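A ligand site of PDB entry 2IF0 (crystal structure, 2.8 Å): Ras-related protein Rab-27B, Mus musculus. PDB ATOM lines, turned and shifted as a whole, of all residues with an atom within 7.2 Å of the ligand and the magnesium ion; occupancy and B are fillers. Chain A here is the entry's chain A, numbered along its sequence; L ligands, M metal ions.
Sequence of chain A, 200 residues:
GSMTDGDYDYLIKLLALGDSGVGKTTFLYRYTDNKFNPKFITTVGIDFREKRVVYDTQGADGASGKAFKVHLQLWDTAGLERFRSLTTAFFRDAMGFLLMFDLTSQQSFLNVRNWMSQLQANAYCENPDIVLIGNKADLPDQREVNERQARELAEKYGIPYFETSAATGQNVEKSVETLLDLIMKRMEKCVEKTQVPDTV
An oxygen (O5) of the ligand sits at hydrogen-bond distance from the backbone NH (N) of Thr 25 (3.4 Å). O5 of the ligand lies within hydrogen-bond range of N of Thr 26 (3.0 Å). The side-chain hydroxyl (OG1) of Thr 26 is in hydrogen-bond range of an oxygen (O5) of the ligand (2.6 Å). The backbone NH of Lys 24 sits at hydrogen-bond distance from an oxygen (O3) of the ligand (2.8 Å). An oxygen (O3) of the ligand is in salt-bridge range of the side-chain amino group of Lys 24. N of Ala 166 lies within hydrogen-bond range of O11 of the ligand (2.7 Å). The side-chain carboxylate (OD1) of Asp 138 lies within hydrogen-bond range of a nitrogen (N3) of the ligand (2.8 Å). N of Gly 23 lies within hydrogen-bond range of O3 of the ligand, at 2.9 Å. The backbone NH (N) of Gly 21 lies within hydrogen-bond range of an oxygen (O2) of the ligand, at 2.9 Å. An oxygen (O8) of the ligand sits at hydrogen-bond distance from the side-chain amino group (NZ) of Lys 136 (3.0 Å). The side-chain amide nitrogen (ND2) of Asn 135 lies within hydrogen-bond range of a nitrogen (N2) of the ligand. The backbone NH of Val 22 lies within hydrogen-bond range of an oxygen (O3) of the ligand (3.4 Å).
O of Asp 19 lies within hydrogen-bond range of NZ of Lys 24 (2.5 Å). The backbone NH (N) of Ala 166 lies within hydrogen-bond range of the side-chain amide oxygen (OD1) of Asn 135 (3.4 Å). The side-chain carboxylate (OD1) of Asp 138 sits at hydrogen-bond distance from the side-chain hydroxyl (OG) of Ser 165, at 2.5 Å. The side-chain amino group of Lys 136 lies within hydrogen-bond range of the backbone carbonyl oxygen of Gly 21 (3.0 Å). The backbone carbonyl oxygen of Thr 164 is in hydrogen-bond range of the backbone NH of Lys 136 (3.1 Å). The side-chain carboxylate (OD1) of Asp 102 lies within salt-bridge range of the side-chain amino group (NZ) of Lys 136 (3.3 Å). ND2 of Asn 135 is in hydrogen-bond range of O of Val 22 (2.7 Å). The side-chain hydroxyl of Ser 165 is in hydrogen-bond range of the backbone NH of Thr 168, at 3.1 Å.
Asp 19 touches the ligand (O to O3, 3.7 Å). Ser 20 touches the ligand. Leu 139 touches the ligand (CD1 to N4, 3.6 Å). Ser 165 touches the ligand (C to O11, 3.4 Å). Ala 167 touches the ligand.
Of the 27 residues printed, 1 comes within 4 Å of the magnesium ion.
The magnesium ion is bound by an oxygen (O1) of the ligand and the side-chain hydroxyl of Thr 25. The magnesium ion has two donor atoms within binding distance.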
ATOM      1  N   LEU A  17      31.108  10.005  -2.445  1.00  0.00           N
ATOM      2  CA  LEU A  17      31.683  11.311  -2.755  1.00  0.00           C
ATOM      3  C   LEU A  17      31.048  11.818  -4.042  1.00  0.00           C
ATOM      4  O   LEU A  17      30.406  11.043  -4.767  1.00  0.00           O
ATOM      5  CB  LEU A  17      33.203  11.213  -2.871  1.00  0.00           C
ATOM      6  CG  LEU A  17      34.025  10.624  -1.709  1.00  0.00           C
ATOM      7  CD1 LEU A  17      35.497  10.565  -2.055  1.00  0.00           C
ATOM      8  CD2 LEU A  17      33.827  11.383  -0.410  1.00  0.00           C
ATOM      9  N   GLY A  18      31.219  13.100  -4.328  1.00  0.00           N
ATOM     10  CA  GLY A  18      30.694  13.721  -5.547  1.00  0.00           C
ATOM     11  C   GLY A  18      29.932  14.999  -5.273  1.00  0.00           C
ATOM     12  O   GLY A  18      29.492  15.239  -4.134  1.00  0.00           O
ATOM     13  N   ASP A  19      29.785  15.819  -6.311  1.00  0.00           N
ATOM     14  CA  ASP A  19      29.022  17.087  -6.251  1.00  0.00           C
ATOM     15  C   ASP A  19      27.618  16.970  -5.653  1.00  0.00           C
ATOM     16  O   ASP A  19      27.068  15.873  -5.524  1.00  0.00           O
ATOM     17  CB  ASP A  19      28.904  17.695  -7.650  1.00  0.00           C
ATOM     18  CG  ASP A  19      30.202  18.315  -8.147  1.00  0.00           C
ATOM     19  OD1 ASP A  19      30.161  18.936  -9.233  1.00  0.00           O
ATOM     20  OD2 ASP A  19      31.251  18.196  -7.470  1.00  0.00           O
ATOM     21  N   SER A  20      27.029  18.112  -5.303  1.00  0.00           N
ATOM     22  CA  SER A  20      25.642  18.153  -4.855  1.00  0.00           C
ATOM     23  C   SER A  20      24.699  17.817  -6.005  1.00  0.00           C
ATOM     24  O   SER A  20      24.942  18.192  -7.159  1.00  0.00           O
ATOM     25  CB  SER A  20      25.298  19.518  -4.301  1.00  0.00           C
ATOM     26  OG  SER A  20      26.186  19.853  -3.251  1.00  0.00           O
ATOM     27  N   GLY A  21      23.623  17.101  -5.688  1.00  0.00           N
ATOM     28  CA  GLY A  21      22.584  16.803  -6.667  1.00  0.00           C
ATOM     29  C   GLY A  21      22.982  15.722  -7.646  1.00  0.00           C
ATOM     30  O   GLY A  21      22.271  15.450  -8.604  1.00  0.00           O
ATOM     31  N   VAL A  22      24.130  15.106  -7.397  1.00  0.00           N
ATOM     32  CA  VAL A  22      24.645  14.020  -8.210  1.00  0.00           C
ATOM     33  C   VAL A  22      23.850  12.743  -7.985  1.00  0.00           C
ATOM     34  O   VAL A  22      23.644  11.959  -8.924  1.00  0.00           O
ATOM     35  CB  VAL A  22      26.198  13.860  -7.961  1.00  0.00           C
ATOM     36  CG1 VAL A  22      26.602  12.439  -7.625  1.00  0.00           C
ATOM     37  CG2 VAL A  22      26.972  14.389  -9.137  1.00  0.00           C
ATOM     38  N   GLY A  23      23.372  12.545  -6.757  1.00  0.00           N
ATOM     39  CA  GLY A  23      22.509  11.414  -6.427  1.00  0.00           C
ATOM     40  C   GLY A  23      23.046  10.486  -5.353  1.00  0.00           C
ATOM     41  O   GLY A  23      22.565   9.367  -5.223  1.00  0.00           O
ATOM     42  N   LYS A  24      24.017  10.958  -4.580  1.00  0.00           N
ATOM     43  CA  LYS A  24      24.674  10.146  -3.548  1.00  0.00           C
ATOM     44  C   LYS A  24      23.673   9.572  -2.543  1.00  0.00           C
ATOM     45  O   LYS A  24      23.646   8.363  -2.311  1.00  0.00           O
ATOM     46  CB  LYS A  24      25.744  10.945  -2.805  1.00  0.00           C
ATOM     47  CG  LYS A  24      26.770  11.616  -3.685  1.00  0.00           C
ATOM     48  CD  LYS A  24      27.688  12.508  -2.867  1.00  0.00           C
ATOM     49  CE  LYS A  24      26.949  13.727  -2.299  1.00  0.00           C
ATOM     50  NZ  LYS A  24      26.538  14.695  -3.345  1.00  0.00           N
ATOM     51  N   THR A  25      22.850  10.457  -1.968  1.00  0.00           N
ATOM     52  CA  THR A  25      21.867  10.069  -0.959  1.00  0.00           C
ATOM     53  C   THR A  25      20.804   9.135  -1.546  1.00  0.00           C
ATOM     54  O   THR A  25      20.394   8.180  -0.893  1.00  0.00           O
ATOM     55  CB  THR A  25      21.171  11.299  -0.302  1.00  0.00           C
ATOM     56  OG1 THR A  25      22.146  12.319  -0.019  1.00  0.00           O
ATOM     57  CG2 THR A  25      20.461  10.918   0.979  1.00  0.00           C
ATOM     58  N   THR A  26      20.373   9.397  -2.777  1.00  0.00           N
ATOM     59  CA  THR A  26      19.364   8.559  -3.426  1.00  0.00           C
ATOM     60  C   THR A  26      19.936   7.194  -3.819  1.00  0.00           C
ATOM     61  O   THR A  26      19.245   6.186  -3.743  1.00  0.00           O
ATOM     62  CB  THR A  26      18.729   9.220  -4.674  1.00  0.00           C
ATOM     63  OG1 THR A  26      18.633  10.634  -4.500  1.00  0.00           O
ATOM     64  CG2 THR A  26      17.336   8.649  -4.908  1.00  0.00           C
ATOM     65  N   PHE A  27      21.202   7.185  -4.247  1.00  0.00           N
ATOM     66  CA  PHE A  27      21.922   5.957  -4.616  1.00  0.00           C
ATOM     67  C   PHE A  27      22.065   5.059  -3.397  1.00  0.00           C
ATOM     68  O   PHE A  27      21.805   3.855  -3.475  1.00  0.00           O
ATOM     69  CB  PHE A  27      23.306   6.337  -5.177  1.00  0.00           C
ATOM     70  CG  PHE A  27      24.151   5.173  -5.646  1.00  0.00           C
ATOM     71  CD1 PHE A  27      24.361   4.959  -7.003  1.00  0.00           C
ATOM     72  CD2 PHE A  27      24.801   4.333  -4.735  1.00  0.00           C
ATOM     73  CE1 PHE A  27      25.167   3.908  -7.443  1.00  0.00           C
ATOM     74  CE2 PHE A  27      25.605   3.278  -5.166  1.00  0.00           C
ATOM     75  CZ  PHE A  27      25.798   3.064  -6.517  1.00  0.00           C
ATOM     76  N   LEU A  28      22.456   5.645  -2.268  1.00  0.00           N
ATOM     77  CA  LEU A  28      22.675   4.893  -1.033  1.00  0.00           C
ATOM     78  C   LEU A  28      21.401   4.273  -0.493  1.00  0.00           C
ATOM     79  O   LEU A  28      21.416   3.144   0.001  1.00  0.00           O
ATOM     80  CB  LEU A  28      23.296   5.793   0.035  1.00  0.00           C
ATOM     81  CG  LEU A  28      24.758   6.186  -0.166  1.00  0.00           C
ATOM     82  CD1 LEU A  28      25.255   6.955   1.029  1.00  0.00           C
ATOM     83  CD2 LEU A  28      25.624   4.949  -0.419  1.00  0.00           C
ATOM     84  N   MET A 100      31.114   9.359  -7.571  1.00  0.00           N
ATOM     85  CA  MET A 100      30.058   9.529  -8.562  1.00  0.00           C
ATOM     86  C   MET A 100      29.965  10.908  -9.171  1.00  0.00           C
ATOM     87  O   MET A 100      30.339  11.909  -8.570  1.00  0.00           O
ATOM     88  CB  MET A 100      28.694   9.043  -8.047  1.00  0.00           C
ATOM     89  CG  MET A 100      28.342   9.378  -6.610  1.00  0.00           C
ATOM     90  SD  MET A 100      27.141   8.213  -5.924  1.00  0.00           S
ATOM     91  CE  MET A 100      25.721   8.540  -6.988  1.00  0.00           C
ATOM     92  N   ASP A 102      27.363  12.995 -12.468  1.00  0.00           N
ATOM     93  CA  ASP A 102      26.072  12.987 -13.138  1.00  0.00           C
ATOM     94  C   ASP A 102      26.293  12.985 -14.633  1.00  0.00           C
ATOM     95  O   ASP A 102      26.888  13.900 -15.195  1.00  0.00           O
ATOM     96  CB  ASP A 102      25.263  14.214 -12.695  1.00  0.00           C
ATOM     97  CG  ASP A 102      23.816  14.155 -13.129  1.00  0.00           C
ATOM     98  OD1 ASP A 102      23.001  14.832 -12.478  1.00  0.00           O
ATOM     99  OD2 ASP A 102      23.478  13.480 -14.131  1.00  0.00           O
ATOM    100  N   ASN A 135      26.101   8.471 -12.637  1.00  0.00           N
ATOM    101  CA  ASN A 135      24.729   8.319 -12.183  1.00  0.00           C
ATOM    102  C   ASN A 135      23.722   8.947 -13.146  1.00  0.00           C
ATOM    103  O   ASN A 135      24.094   9.723 -14.038  1.00  0.00           O
ATOM    104  CB  ASN A 135      24.574   8.909 -10.788  1.00  0.00           C
ATOM    105  CG  ASN A 135      23.251   8.563 -10.144  1.00  0.00           C
ATOM    106  OD1 ASN A 135      22.811   7.415 -10.200  1.00  0.00           O
ATOM    107  ND2 ASN A 135      22.614   9.553  -9.524  1.00  0.00           N
ATOM    108  N   LYS A 136      22.452   8.616 -12.942  1.00  0.00           N
ATOM    109  CA  LYS A 136      21.322   9.137 -13.731  1.00  0.00           C
ATOM    110  C   LYS A 136      21.364   8.650 -15.173  1.00  0.00           C
ATOM    111  O   LYS A 136      21.127   9.415 -16.118  1.00  0.00           O
ATOM    112  CB  LYS A 136      21.236  10.662 -13.639  1.00  0.00           C
ATOM    113  CG  LYS A 136      21.125  11.199 -12.219  1.00  0.00           C
ATOM    114  CD  LYS A 136      20.784  12.670 -12.195  1.00  0.00           C
ATOM    115  CE  LYS A 136      20.948  13.239 -10.793  1.00  0.00           C
ATOM    116  NZ  LYS A 136      20.292  14.572 -10.665  1.00  0.00           N
ATOM    117  N   ALA A 137      21.659   7.358 -15.336  1.00  0.00           N
ATOM    118  CA  ALA A 137      21.724   6.743 -16.658  1.00  0.00           C
ATOM    119  C   ALA A 137      20.349   6.601 -17.317  1.00  0.00           C
ATOM    120  O   ALA A 137      20.255   6.254 -18.483  1.00  0.00           O
ATOM    121  CB  ALA A 137      22.427   5.393 -16.591  1.00  0.00           C
ATOM    122  N   ASP A 138      19.286   6.894 -16.565  1.00  0.00           N
ATOM    123  CA  ASP A 138      17.913   6.743 -17.065  1.00  0.00           C
ATOM    124  C   ASP A 138      17.370   7.995 -17.751  1.00  0.00           C
ATOM    125  O   ASP A 138      16.180   8.059 -18.061  1.00  0.00           O
ATOM    126  CB  ASP A 138      16.983   6.356 -15.910  1.00  0.00           C
ATOM    127  CG  ASP A 138      17.076   7.326 -14.769  1.00  0.00           C
ATOM    128  OD1 ASP A 138      18.095   7.285 -14.053  1.00  0.00           O
ATOM    129  OD2 ASP A 138      16.157   8.138 -14.588  1.00  0.00           O
ATOM    130  N   LEU A 139      18.234   8.985 -17.998  1.00  0.00           N
ATOM    131  CA  LEU A 139      17.817  10.189 -18.723  1.00  0.00           C
ATOM    132  C   LEU A 139      18.759  10.437 -19.906  1.00  0.00           C
ATOM    133  O   LEU A 139      19.532  11.396 -19.897  1.00  0.00           O
ATOM    134  CB  LEU A 139      17.782  11.412 -17.806  1.00  0.00           C
ATOM    135  CG  LEU A 139      17.066  11.348 -16.443  1.00  0.00           C
ATOM    136  CD1 LEU A 139      17.355  12.610 -15.640  1.00  0.00           C
ATOM    137  CD2 LEU A 139      15.567  11.116 -16.584  1.00  0.00           C
ATOM    138  N   GLN A 142      19.203  13.866 -21.630  1.00  0.00           N
ATOM    139  CA  GLN A 142      19.870  14.932 -20.884  1.00  0.00           C
ATOM    140  C   GLN A 142      21.369  14.710 -20.731  1.00  0.00           C
ATOM    141  O   GLN A 142      22.073  15.571 -20.187  1.00  0.00           O
ATOM    142  CB  GLN A 142      19.246  15.079 -19.493  1.00  0.00           C
ATOM    143  CG  GLN A 142      17.742  15.297 -19.476  1.00  0.00           C
ATOM    144  CD  GLN A 142      17.273  15.956 -18.202  1.00  0.00           C
ATOM    145  OE1 GLN A 142      17.905  16.893 -17.694  1.00  0.00           O
ATOM    146  NE2 GLN A 142      16.143  15.491 -17.666  1.00  0.00           N
ATOM    147  N   THR A 164      25.186   3.957 -13.764  1.00  0.00           N
ATOM    148  CA  THR A 164      24.164   3.549 -12.802  1.00  0.00           C
ATOM    149  C   THR A 164      22.953   4.468 -12.786  1.00  0.00           C
ATOM    150  O   THR A 164      23.011   5.613 -13.271  1.00  0.00           O
ATOM    151  CB  THR A 164      24.741   3.549 -11.370  1.00  0.00           C
ATOM    152  OG1 THR A 164      25.121   4.884 -11.011  1.00  0.00           O
ATOM    153  CG2 THR A 164      25.966   2.637 -11.260  1.00  0.00           C
ATOM    154  N   SER A 165      21.862   3.979 -12.213  1.00  0.00           N
ATOM    155  CA  SER A 165      20.663   4.776 -11.996  1.00  0.00           C
ATOM    156  C   SER A 165      20.042   4.473 -10.647  1.00  0.00           C
ATOM    157  O   SER A 165      19.595   3.353 -10.401  1.00  0.00           O
ATOM    158  CB  SER A 165      19.633   4.523 -13.114  1.00  0.00           C
ATOM    159  OG  SER A 165      18.400   5.160 -12.824  1.00  0.00           O
ATOM    160  N   ALA A 166      20.008   5.468  -9.759  1.00  0.00           N
ATOM    161  CA  ALA A 166      19.380   5.314  -8.445  1.00  0.00           C
ATOM    162  C   ALA A 166      17.855   5.143  -8.518  1.00  0.00           C
ATOM    163  O   ALA A 166      17.253   4.566  -7.621  1.00  0.00           O
ATOM    164  CB  ALA A 166      19.741   6.499  -7.561  1.00  0.00           C
ATOM    165  N   ALA A 167      17.258   5.657  -9.592  1.00  0.00           N
ATOM    166  CA  ALA A 167      15.811   5.555  -9.792  1.00  0.00           C
ATOM    167  C   ALA A 167      15.398   4.166 -10.316  1.00  0.00           C
ATOM    168  O   ALA A 167      14.442   3.576  -9.826  1.00  0.00           O
ATOM    169  CB  ALA A 167      15.315   6.668 -10.727  1.00  0.00           C
ATOM    170  N   THR A 168      16.149   3.642 -11.298  1.00  0.00           N
ATOM    171  CA  THR A 168      15.890   2.318 -11.866  1.00  0.00           C
ATOM    172  C   THR A 168      16.518   1.211 -11.022  1.00  0.00           C
ATOM    173  O   THR A 168      15.931   0.131 -10.862  1.00  0.00           O
ATOM    174  CB  THR A 168      16.448   2.181 -13.298  1.00  0.00           C
ATOM    175  OG1 THR A 168      16.011   3.286 -14.089  1.00  0.00           O
ATOM    176  CG2 THR A 168      15.972   0.890 -13.959  1.00  0.00           C
ATOM    177  N   GLY A 169      17.711   1.480 -10.503  1.00  0.00           N
ATOM    178  CA  GLY A 169      18.498   0.477  -9.787  1.00  0.00           C
ATOM    179  C   GLY A 169      19.575  -0.137 -10.677  1.00  0.00           C
ATOM    180  O   GLY A 169      20.317  -1.006 -10.225  1.00  0.00           O
ATOM    181  N   VAL A 172      23.382  -0.461  -9.684  1.00  0.00           N
ATOM    182  CA  VAL A 172      23.541   0.056  -8.320  1.00  0.00           C
ATOM    183  C   VAL A 172      24.192  -1.013  -7.438  1.00  0.00           C
ATOM    184  O   VAL A 172      25.223  -0.761  -6.809  1.00  0.00           O
ATOM    185  CB  VAL A 172      22.200   0.564  -7.711  1.00  0.00           C
ATOM    186  CG1 VAL A 172      22.334   0.792  -6.217  1.00  0.00           C
ATOM    187  CG2 VAL A 172      21.764   1.846  -8.370  1.00  0.00           C
HETATM  188  P1  LIG L   1      23.091  14.303  -3.526  1.00  0.00           P
HETATM  189  O1  LIG L   1      22.831  13.428  -2.317  1.00  0.00           O
HETATM  190  O2  LIG L   1      23.333  15.736  -3.121  1.00  0.00           O
HETATM  191  O3  LIG L   1      24.281  13.731  -4.253  1.00  0.00           O
HETATM  192  O4  LIG L   1      21.848  14.359  -4.532  1.00  0.00           O
HETATM  193  P2  LIG L   1      20.462  13.584  -4.292  1.00  0.00           P
HETATM  194  O5  LIG L   1      20.692  12.134  -3.948  1.00  0.00           O
HETATM  195  O6  LIG L   1      19.629  14.279  -3.243  1.00  0.00           O
HETATM  196  O7  LIG L   1      19.772  13.686  -5.725  1.00  0.00           O
HETATM  197  C1  LIG L   1      19.539  14.968  -6.314  1.00  0.00           C
HETATM  198  C2  LIG L   1      18.289  14.848  -7.175  1.00  0.00           C
HETATM  199  O8  LIG L   1      18.546  14.014  -8.304  1.00  0.00           O
HETATM  200  C3  LIG L   1      17.160  14.198  -6.366  1.00  0.00           C
HETATM  201  O9  LIG L   1      15.966  14.966  -6.535  1.00  0.00           O
HETATM  202  C4  LIG L   1      17.007  12.806  -6.942  1.00  0.00           C
HETATM  203  O10 LIG L   1      15.640  12.391  -7.009  1.00  0.00           O
HETATM  204  C5  LIG L   1      17.616  12.922  -8.327  1.00  0.00           C
HETATM  205  N1  LIG L   1      18.307  11.663  -8.686  1.00  0.00           N
HETATM  206  C6  LIG L   1      19.245  11.038  -7.955  1.00  0.00           C
HETATM  207  N2  LIG L   1      19.653   9.909  -8.582  1.00  0.00           N
HETATM  208  C7  LIG L   1      18.978   9.809  -9.736  1.00  0.00           C
HETATM  209  C8  LIG L   1      18.928   8.865 -10.884  1.00  0.00           C
HETATM  210  O11 LIG L   1      19.658   7.851 -10.902  1.00  0.00           O
HETATM  211  N3  LIG L   1      18.079   9.132 -11.886  1.00  0.00           N
HETATM  212  C9  LIG L   1      17.277  10.216 -11.881  1.00  0.00           C
HETATM  213  N4  LIG L   1      16.450  10.439 -12.932  1.00  0.00           N
HETATM  214  N5  LIG L   1      17.275  11.123 -10.874  1.00  0.00           N
HETATM  215  C10 LIG L   1      18.081  10.975  -9.795  1.00  0.00           C
HETATM  216 MG    MG M   1      21.809  14.355  -0.965  1.00  0.00          MG
